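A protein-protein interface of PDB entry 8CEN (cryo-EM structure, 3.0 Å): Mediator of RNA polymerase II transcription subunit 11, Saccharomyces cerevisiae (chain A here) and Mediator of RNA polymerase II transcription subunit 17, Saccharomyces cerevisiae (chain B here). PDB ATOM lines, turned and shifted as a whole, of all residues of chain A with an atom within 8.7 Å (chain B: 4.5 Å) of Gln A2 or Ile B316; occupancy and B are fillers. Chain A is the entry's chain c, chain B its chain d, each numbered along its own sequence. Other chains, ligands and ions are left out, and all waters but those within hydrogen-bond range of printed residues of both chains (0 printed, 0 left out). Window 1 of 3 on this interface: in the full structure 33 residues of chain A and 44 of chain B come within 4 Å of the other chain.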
ATOM      1  N   MET A   1     -16.975 -15.517   8.628  1.00  0.00           N
ATOM      2  CA  MET A   1     -17.163 -16.183   9.907  1.00  0.00           C
ATOM      3  C   MET A   1     -16.539 -15.296  10.982  1.00  0.00           C
ATOM      4  O   MET A   1     -17.246 -14.664  11.764  1.00  0.00           O
ATOM      5  CB  MET A   1     -16.532 -17.573   9.880  1.00  0.00           C
ATOM      6  CG  MET A   1     -16.479 -18.263  11.219  1.00  0.00           C
ATOM      7  SD  MET A   1     -18.055 -19.072  11.509  1.00  0.00           S
ATOM      8  CE  MET A   1     -17.673 -20.027  12.960  1.00  0.00           C
ATOM      9  N   GLN A   2     -15.207 -15.272  11.022  1.00  0.00           N
ATOM     10  CA  GLN A   2     -14.442 -14.195  11.629  1.00  0.00           C
ATOM     11  C   GLN A   2     -14.166 -13.105  10.595  1.00  0.00           C
ATOM     12  O   GLN A   2     -14.193 -13.371   9.390  1.00  0.00           O
ATOM     13  CB  GLN A   2     -13.132 -14.730  12.203  1.00  0.00           C
ATOM     14  CG  GLN A   2     -13.327 -15.675  13.361  1.00  0.00           C
ATOM     15  CD  GLN A   2     -13.994 -14.971  14.529  1.00  0.00           C
ATOM     16  OE1 GLN A   2     -15.154 -15.221  14.847  1.00  0.00           O
ATOM     17  NE2 GLN A   2     -13.259 -14.068  15.163  1.00  0.00           N
ATOM     18  N   PRO A   3     -13.939 -11.867  11.035  1.00  0.00           N
ATOM     19  CA  PRO A   3     -13.567 -10.796  10.096  1.00  0.00           C
ATOM     20  C   PRO A   3     -12.263 -11.100   9.379  1.00  0.00           C
ATOM     21  O   PRO A   3     -11.334 -11.683   9.966  1.00  0.00           O
ATOM     22  CB  PRO A   3     -13.428  -9.563  11.002  1.00  0.00           C
ATOM     23  CG  PRO A   3     -14.288  -9.860  12.177  1.00  0.00           C
ATOM     24  CD  PRO A   3     -14.190 -11.340  12.391  1.00  0.00           C
ATOM     25  N   PRO A   4     -12.167 -10.722   8.097  1.00  0.00           N
ATOM     26  CA  PRO A   4     -10.914 -10.938   7.348  1.00  0.00           C
ATOM     27  C   PRO A   4      -9.710 -10.222   7.936  1.00  0.00           C
ATOM     28  O   PRO A   4      -8.584 -10.688   7.745  1.00  0.00           O
ATOM     29  CB  PRO A   4     -11.254 -10.414   5.946  1.00  0.00           C
ATOM     30  CG  PRO A   4     -12.742 -10.508   5.854  1.00  0.00           C
ATOM     31  CD  PRO A   4     -13.242 -10.204   7.235  1.00  0.00           C
ATOM     32  N   TYR A   5      -9.909  -9.108   8.646  1.00  0.00           N
ATOM     33  CA  TYR A   5      -8.799  -8.458   9.342  1.00  0.00           C
ATOM     34  C   TYR A   5      -8.266  -9.332  10.472  1.00  0.00           C
ATOM     35  O   TYR A   5      -7.047  -9.437  10.663  1.00  0.00           O
ATOM     36  CB  TYR A   5      -9.241  -7.105   9.880  1.00  0.00           C
ATOM     37  CG  TYR A   5      -8.137  -6.083  10.021  1.00  0.00           C
ATOM     38  CD1 TYR A   5      -7.245  -6.133  11.087  1.00  0.00           C
ATOM     39  CD2 TYR A   5      -7.988  -5.058   9.093  1.00  0.00           C
ATOM     40  CE1 TYR A   5      -6.232  -5.197  11.221  1.00  0.00           C
ATOM     41  CE2 TYR A   5      -6.978  -4.117   9.217  1.00  0.00           C
ATOM     42  CZ  TYR A   5      -6.105  -4.191  10.282  1.00  0.00           C
ATOM     43  OH  TYR A   5      -5.105  -3.252  10.400  1.00  0.00           O
ATOM     44  N   ILE A   6      -9.166  -9.958  11.236  1.00  0.00           N
ATOM     45  CA  ILE A   6      -8.750 -10.896  12.276  1.00  0.00           C
ATOM     46  C   ILE A   6      -8.037 -12.090  11.656  1.00  0.00           C
ATOM     47  O   ILE A   6      -7.026 -12.568  12.185  1.00  0.00           O
ATOM     48  CB  ILE A   6      -9.962 -11.335  13.124  1.00  0.00           C
ATOM     49  CG1 ILE A   6     -10.801 -10.126  13.546  1.00  0.00           C
ATOM     50  CG2 ILE A   6      -9.510 -12.114  14.352  1.00  0.00           C
ATOM     51  CD1 ILE A   6     -10.070  -9.145  14.446  1.00  0.00           C
ATOM     52  N   GLN A   7      -8.545 -12.576  10.516  1.00  0.00           N
ATOM     53  CA  GLN A   7      -7.885 -13.674   9.809  1.00  0.00           C
ATOM     54  C   GLN A   7      -6.477 -13.286   9.370  1.00  0.00           C
ATOM     55  O   GLN A   7      -5.524 -14.054   9.548  1.00  0.00           O
ATOM     56  CB  GLN A   7      -8.721 -14.106   8.603  1.00  0.00           C
ATOM     57  CG  GLN A   7     -10.131 -14.546   8.947  1.00  0.00           C
ATOM     58  CD  GLN A   7     -10.192 -15.990   9.403  1.00  0.00           C
ATOM     59  OE1 GLN A   7      -9.818 -16.307  10.529  1.00  0.00           O
ATOM     60  NE2 GLN A   7     -10.683 -16.869   8.536  1.00  0.00           N
ATOM     61  N   GLU A   8      -6.329 -12.081   8.808  1.00  0.00           N
ATOM     62  CA  GLU A   8      -5.028 -11.620   8.331  1.00  0.00           C
ATOM     63  C   GLU A   8      -4.045 -11.437   9.480  1.00  0.00           C
ATOM     64  O   GLU A   8      -2.866 -11.782   9.349  1.00  0.00           O
ATOM     65  CB  GLU A   8      -5.185 -10.315   7.551  1.00  0.00           C
ATOM     66  CG  GLU A   8      -5.756 -10.487   6.152  1.00  0.00           C
ATOM     67  CD  GLU A   8      -6.042  -9.162   5.473  1.00  0.00           C
ATOM     68  OE1 GLU A   8      -5.345  -8.173   5.783  1.00  0.00           O
ATOM     69  OE2 GLU A   8      -6.972  -9.106   4.642  1.00  0.00           O
ATOM     70  N   LEU A  10      -4.147 -13.052  12.378  1.00  0.00           N
ATOM     71  CA  LEU A  10      -3.815 -14.399  12.840  1.00  0.00           C
ATOM     72  C   LEU A  10      -2.775 -15.055  11.947  1.00  0.00           C
ATOM     73  O   LEU A  10      -1.823 -15.670  12.441  1.00  0.00           O
ATOM     74  CB  LEU A  10      -5.079 -15.256  12.913  1.00  0.00           C
ATOM     75  CG  LEU A  10      -5.797 -15.371  14.255  1.00  0.00           C
ATOM     76  CD1 LEU A  10      -4.996 -16.272  15.155  1.00  0.00           C
ATOM     77  CD2 LEU A  10      -5.968 -14.021  14.929  1.00  0.00           C
ATOM     78  N   LYS A  88     -17.725  -9.659  27.630  1.00  0.00           N
ATOM     79  CA  LYS A  88     -18.867  -9.361  26.781  1.00  0.00           C
ATOM     80  C   LYS A  88     -20.097 -10.142  27.237  1.00  0.00           C
ATOM     81  O   LYS A  88     -20.047 -10.969  28.151  1.00  0.00           O
ATOM     82  CB  LYS A  88     -18.541  -9.676  25.322  1.00  0.00           C
ATOM     83  CG  LYS A  88     -17.479  -8.778  24.713  1.00  0.00           C
ATOM     84  CD  LYS A  88     -17.325  -9.039  23.222  1.00  0.00           C
ATOM     85  CE  LYS A  88     -16.608 -10.353  22.960  1.00  0.00           C
ATOM     86  NZ  LYS A  88     -16.352 -10.571  21.507  1.00  0.00           N
ATOM     87  N   ILE B 312      -9.675 -22.646  15.955  1.00  0.00           N
ATOM     88  CA  ILE B 312     -10.404 -21.578  16.637  1.00  0.00           C
ATOM     89  C   ILE B 312     -11.075 -20.656  15.626  1.00  0.00           C
ATOM     90  O   ILE B 312     -12.260 -20.326  15.756  1.00  0.00           O
ATOM     91  CB  ILE B 312      -9.460 -20.792  17.569  1.00  0.00           C
ATOM     92  CG1 ILE B 312      -9.272 -21.523  18.894  1.00  0.00           C
ATOM     93  CG2 ILE B 312      -9.981 -19.374  17.833  1.00  0.00           C
ATOM     94  CD1 ILE B 312      -8.333 -20.805  19.825  1.00  0.00           C
ATOM     95  N   MET B 313     -10.344 -20.249  14.590  1.00  0.00           N
ATOM     96  CA  MET B 313     -10.899 -19.265  13.667  1.00  0.00           C
ATOM     97  C   MET B 313     -11.890 -19.890  12.688  1.00  0.00           C
ATOM     98  O   MET B 313     -12.775 -19.196  12.176  1.00  0.00           O
ATOM     99  CB  MET B 313      -9.775 -18.521  12.957  1.00  0.00           C
ATOM    100  CG  MET B 313      -8.985 -17.712  13.963  1.00  0.00           C
ATOM    101  SD  MET B 313     -10.043 -16.449  14.701  1.00  0.00           S
ATOM    102  CE  MET B 313      -8.994 -15.810  15.997  1.00  0.00           C
ATOM    103  N   GLN B 314     -11.761 -21.187  12.398  1.00  0.00           N
ATOM    104  CA  GLN B 314     -12.811 -21.867  11.646  1.00  0.00           C
ATOM    105  C   GLN B 314     -13.972 -22.334  12.517  1.00  0.00           C
ATOM    106  O   GLN B 314     -14.980 -22.798  11.974  1.00  0.00           O
ATOM    107  CB  GLN B 314     -12.259 -23.077  10.886  1.00  0.00           C
ATOM    108  CG  GLN B 314     -11.293 -22.766   9.759  1.00  0.00           C
ATOM    109  CD  GLN B 314     -10.789 -24.029   9.081  1.00  0.00           C
ATOM    110  OE1 GLN B 314     -11.113 -25.142   9.498  1.00  0.00           O
ATOM    111  NE2 GLN B 314     -10.009 -23.862   8.018  1.00  0.00           N
ATOM    112  N   SER B 315     -13.858 -22.238  13.840  1.00  0.00           N
ATOM    113  CA  SER B 315     -14.862 -22.771  14.749  1.00  0.00           C
ATOM    114  C   SER B 315     -15.723 -21.704  15.407  1.00  0.00           C
ATOM    115  O   SER B 315     -16.943 -21.864  15.504  1.00  0.00           O
ATOM    116  CB  SER B 315     -14.163 -23.606  15.832  1.00  0.00           C
ATOM    117  OG  SER B 315     -13.495 -22.772  16.760  1.00  0.00           O
ATOM    118  N   ILE B 316     -15.116 -20.637  15.884  1.00  0.00           N
ATOM    119  CA  ILE B 316     -15.790 -19.634  16.700  1.00  0.00           C
ATOM    120  C   ILE B 316     -16.251 -18.487  15.813  1.00  0.00           C
ATOM    121  O   ILE B 316     -15.501 -18.010  14.955  1.00  0.00           O
ATOM    122  CB  ILE B 316     -14.852 -19.135  17.817  1.00  0.00           C
ATOM    123  CG1 ILE B 316     -14.438 -20.289  18.734  1.00  0.00           C
ATOM    124  CG2 ILE B 316     -15.509 -18.039  18.630  1.00  0.00           C
ATOM    125  CD1 ILE B 316     -15.598 -21.136  19.226  1.00  0.00           C
ATOM    126  N   SER B 317     -17.493 -18.053  16.006  1.00  0.00           N
ATOM    127  CA  SER B 317     -18.010 -16.849  15.376  1.00  0.00           C
ATOM    128  C   SER B 317     -17.871 -15.661  16.325  1.00  0.00           C
ATOM    129  O   SER B 317     -17.673 -15.814  17.532  1.00  0.00           O
ATOM    130  CB  SER B 317     -19.474 -17.038  14.968  1.00  0.00           C
ATOM    131  OG  SER B 317     -20.313 -17.105  16.110  1.00  0.00           O
ATOM    132  N   ASN B 318     -17.987 -14.457  15.760  1.00  0.00           N
ATOM    133  CA  ASN B 318     -17.900 -13.240  16.560  1.00  0.00           C
ATOM    134  C   ASN B 318     -19.123 -13.033  17.442  1.00  0.00           C
ATOM    135  O   ASN B 318     -19.058 -12.255  18.400  1.00  0.00           O
ATOM    136  CB  ASN B 318     -17.712 -12.024  15.652  1.00  0.00           C
ATOM    137  CG  ASN B 318     -16.896 -10.927  16.307  1.00  0.00           C
ATOM    138  OD1 ASN B 318     -16.592 -10.989  17.498  1.00  0.00           O
ATOM    139  ND2 ASN B 318     -16.535  -9.915  15.528  1.00  0.00           N
ATOM    140  N   ASP B 320     -20.366 -15.371  19.317  1.00  0.00           N
ATOM    141  CA  ASP B 320     -20.042 -16.092  20.538  1.00  0.00           C
ATOM    142  C   ASP B 320     -19.109 -15.271  21.424  1.00  0.00           C
ATOM    143  O   ASP B 320     -18.353 -14.421  20.949  1.00  0.00           O
ATOM    144  CB  ASP B 320     -19.395 -17.434  20.200  1.00  0.00           C
ATOM    145  CG  ASP B 320     -20.309 -18.333  19.392  1.00  0.00           C
ATOM    146  OD1 ASP B 320     -21.369 -17.853  18.939  1.00  0.00           O
ATOM    147  OD2 ASP B 320     -19.964 -19.519  19.206  1.00  0.00           O
ATOM    148  N   ILE B 322     -16.182 -15.391  24.544  1.00  0.00           N
ATOM    149  CA  ILE B 322     -15.116 -16.188  25.138  1.00  0.00           C
ATOM    150  C   ILE B 322     -14.468 -15.358  26.242  1.00  0.00           C
ATOM    151  O   ILE B 322     -14.367 -14.131  26.136  1.00  0.00           O
ATOM    152  CB  ILE B 322     -14.075 -16.604  24.066  1.00  0.00           C
ATOM    153  CG1 ILE B 322     -14.710 -17.490  23.001  1.00  0.00           C
ATOM    154  CG2 ILE B 322     -12.901 -17.386  24.650  1.00  0.00           C
ATOM    155  CD1 ILE B 322     -13.801 -17.697  21.820  1.00  0.00           C
ATOM    156  N   ILE B 337     -16.223 -20.554  26.633  1.00  0.00           N
ATOM    157  CA  ILE B 337     -17.271 -19.926  25.840  1.00  0.00           C
ATOM    158  C   ILE B 337     -18.552 -19.914  26.662  1.00  0.00           C
ATOM    159  O   ILE B 337     -18.861 -20.879  27.376  1.00  0.00           O
ATOM    160  CB  ILE B 337     -17.451 -20.645  24.482  1.00  0.00           C
ATOM    161  CG1 ILE B 337     -18.430 -19.891  23.579  1.00  0.00           C
ATOM    162  CG2 ILE B 337     -17.854 -22.110  24.641  1.00  0.00           C
ATOM    163  CD1 ILE B 337     -18.413 -20.381  22.152  1.00  0.00           C
ATOM    164  N   ILE B 357     -13.205 -24.683  26.258  1.00  0.00           N
ATOM    165  CA  ILE B 357     -12.820 -25.156  24.935  1.00  0.00           C
ATOM    166  C   ILE B 357     -11.443 -25.794  25.031  1.00  0.00           C
ATOM    167  O   ILE B 357     -10.491 -25.166  25.512  1.00  0.00           O
ATOM    168  CB  ILE B 357     -12.825 -24.009  23.911  1.00  0.00           C
ATOM    169  CG1 ILE B 357     -14.213 -23.367  23.838  1.00  0.00           C
ATOM    170  CG2 ILE B 357     -12.386 -24.512  22.543  1.00  0.00           C
ATOM    171  CD1 ILE B 357     -14.339 -22.288  22.784  1.00  0.00           C
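Printed residues of chain B that touch a printed residue of chain A: Met B313, Gln B314, Ser B315, Ile B316, Ser B317 and Asn B318. Hydrophobic or aromatic side chains of chain B that line the printed part of chain A: Met B313. Of the 10 printed residues of chain A, 4 touch a printed residue of chain B. Printed residues of chain A that touch a printed residue of chain B: Met A1, Gln A2, Gln A7 and Leu A10. Hydrophobic or aromatic side chains of chain A that line the printed part of chain B: Met A1 and Leu A10. Along chain A the printed residues that touch a printed residue of chain B span positions 1 to 10.
Among the printed residues, pairs that only touch across the chains: Gln A2 with Ser B317 (3.1 Å), Met A1 with Ser B315 (3.2 Å), Gln A7 with Met B313 (3.3 Å), Met A1 with Ile B316 (3.5 Å), Gln A2 with Met B313 (3.6 Å), Met A1 with Ser B317 (3.6 Å), Leu A10 with Met B313 (3.7 Å), Met A1 with Met B313 (3.9 Å) and Met A1 with Gln B314 (3.99 Å).
The backbone carbonyl oxygen (O) of Ile B312 lies within hydrogen-bond range of the side-chain hydroxyl (OG) of Ser B315, 2.9 Å away. OG of Ser B317 lies within hydrogen-bond range of OD1 of Asp B320.
The side-chain amide oxygen (OE1) of Gln A2 sits close to the backbone carbonyl oxygen (O) of Ile B316, 2.8 Å away. The backbone NH (N) of Asn B318 lies within hydrogen-bond range of the side-chain amide oxygen (OE1) of Gln A2 (3.1 Å).
Of chain B, only Met B313, Ile B316, Ser B317 and Asn B318 come within 4 Å of Gln A2. Of the printed residues of chain B, Gln A7 touches Met B313 (3.3 Å). Printed residues of chain B within 4 Å of Leu A10: Met B313 (3.7 Å). Lys A88 touches none of the printed residues of chain B. Printed residues of chain A within 4 Å of Gln B314: Met A1. Ser B315 touches just one residue of chain A: Met A1 (3.2 Å). Of chain A, only Met A1 and Gln A2 come within 4 Å of Ile B316. The nearest printed residue of chain B that does not touch Gln A2 is Ile B312 (5.3 Å). The nearest residue of chain A that does not touch Ile B316 is Pro A3 (7.3 Å). The nearest printed residue of chain B that does not touch Gln A7 is Gln B314 (5.6 Å).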
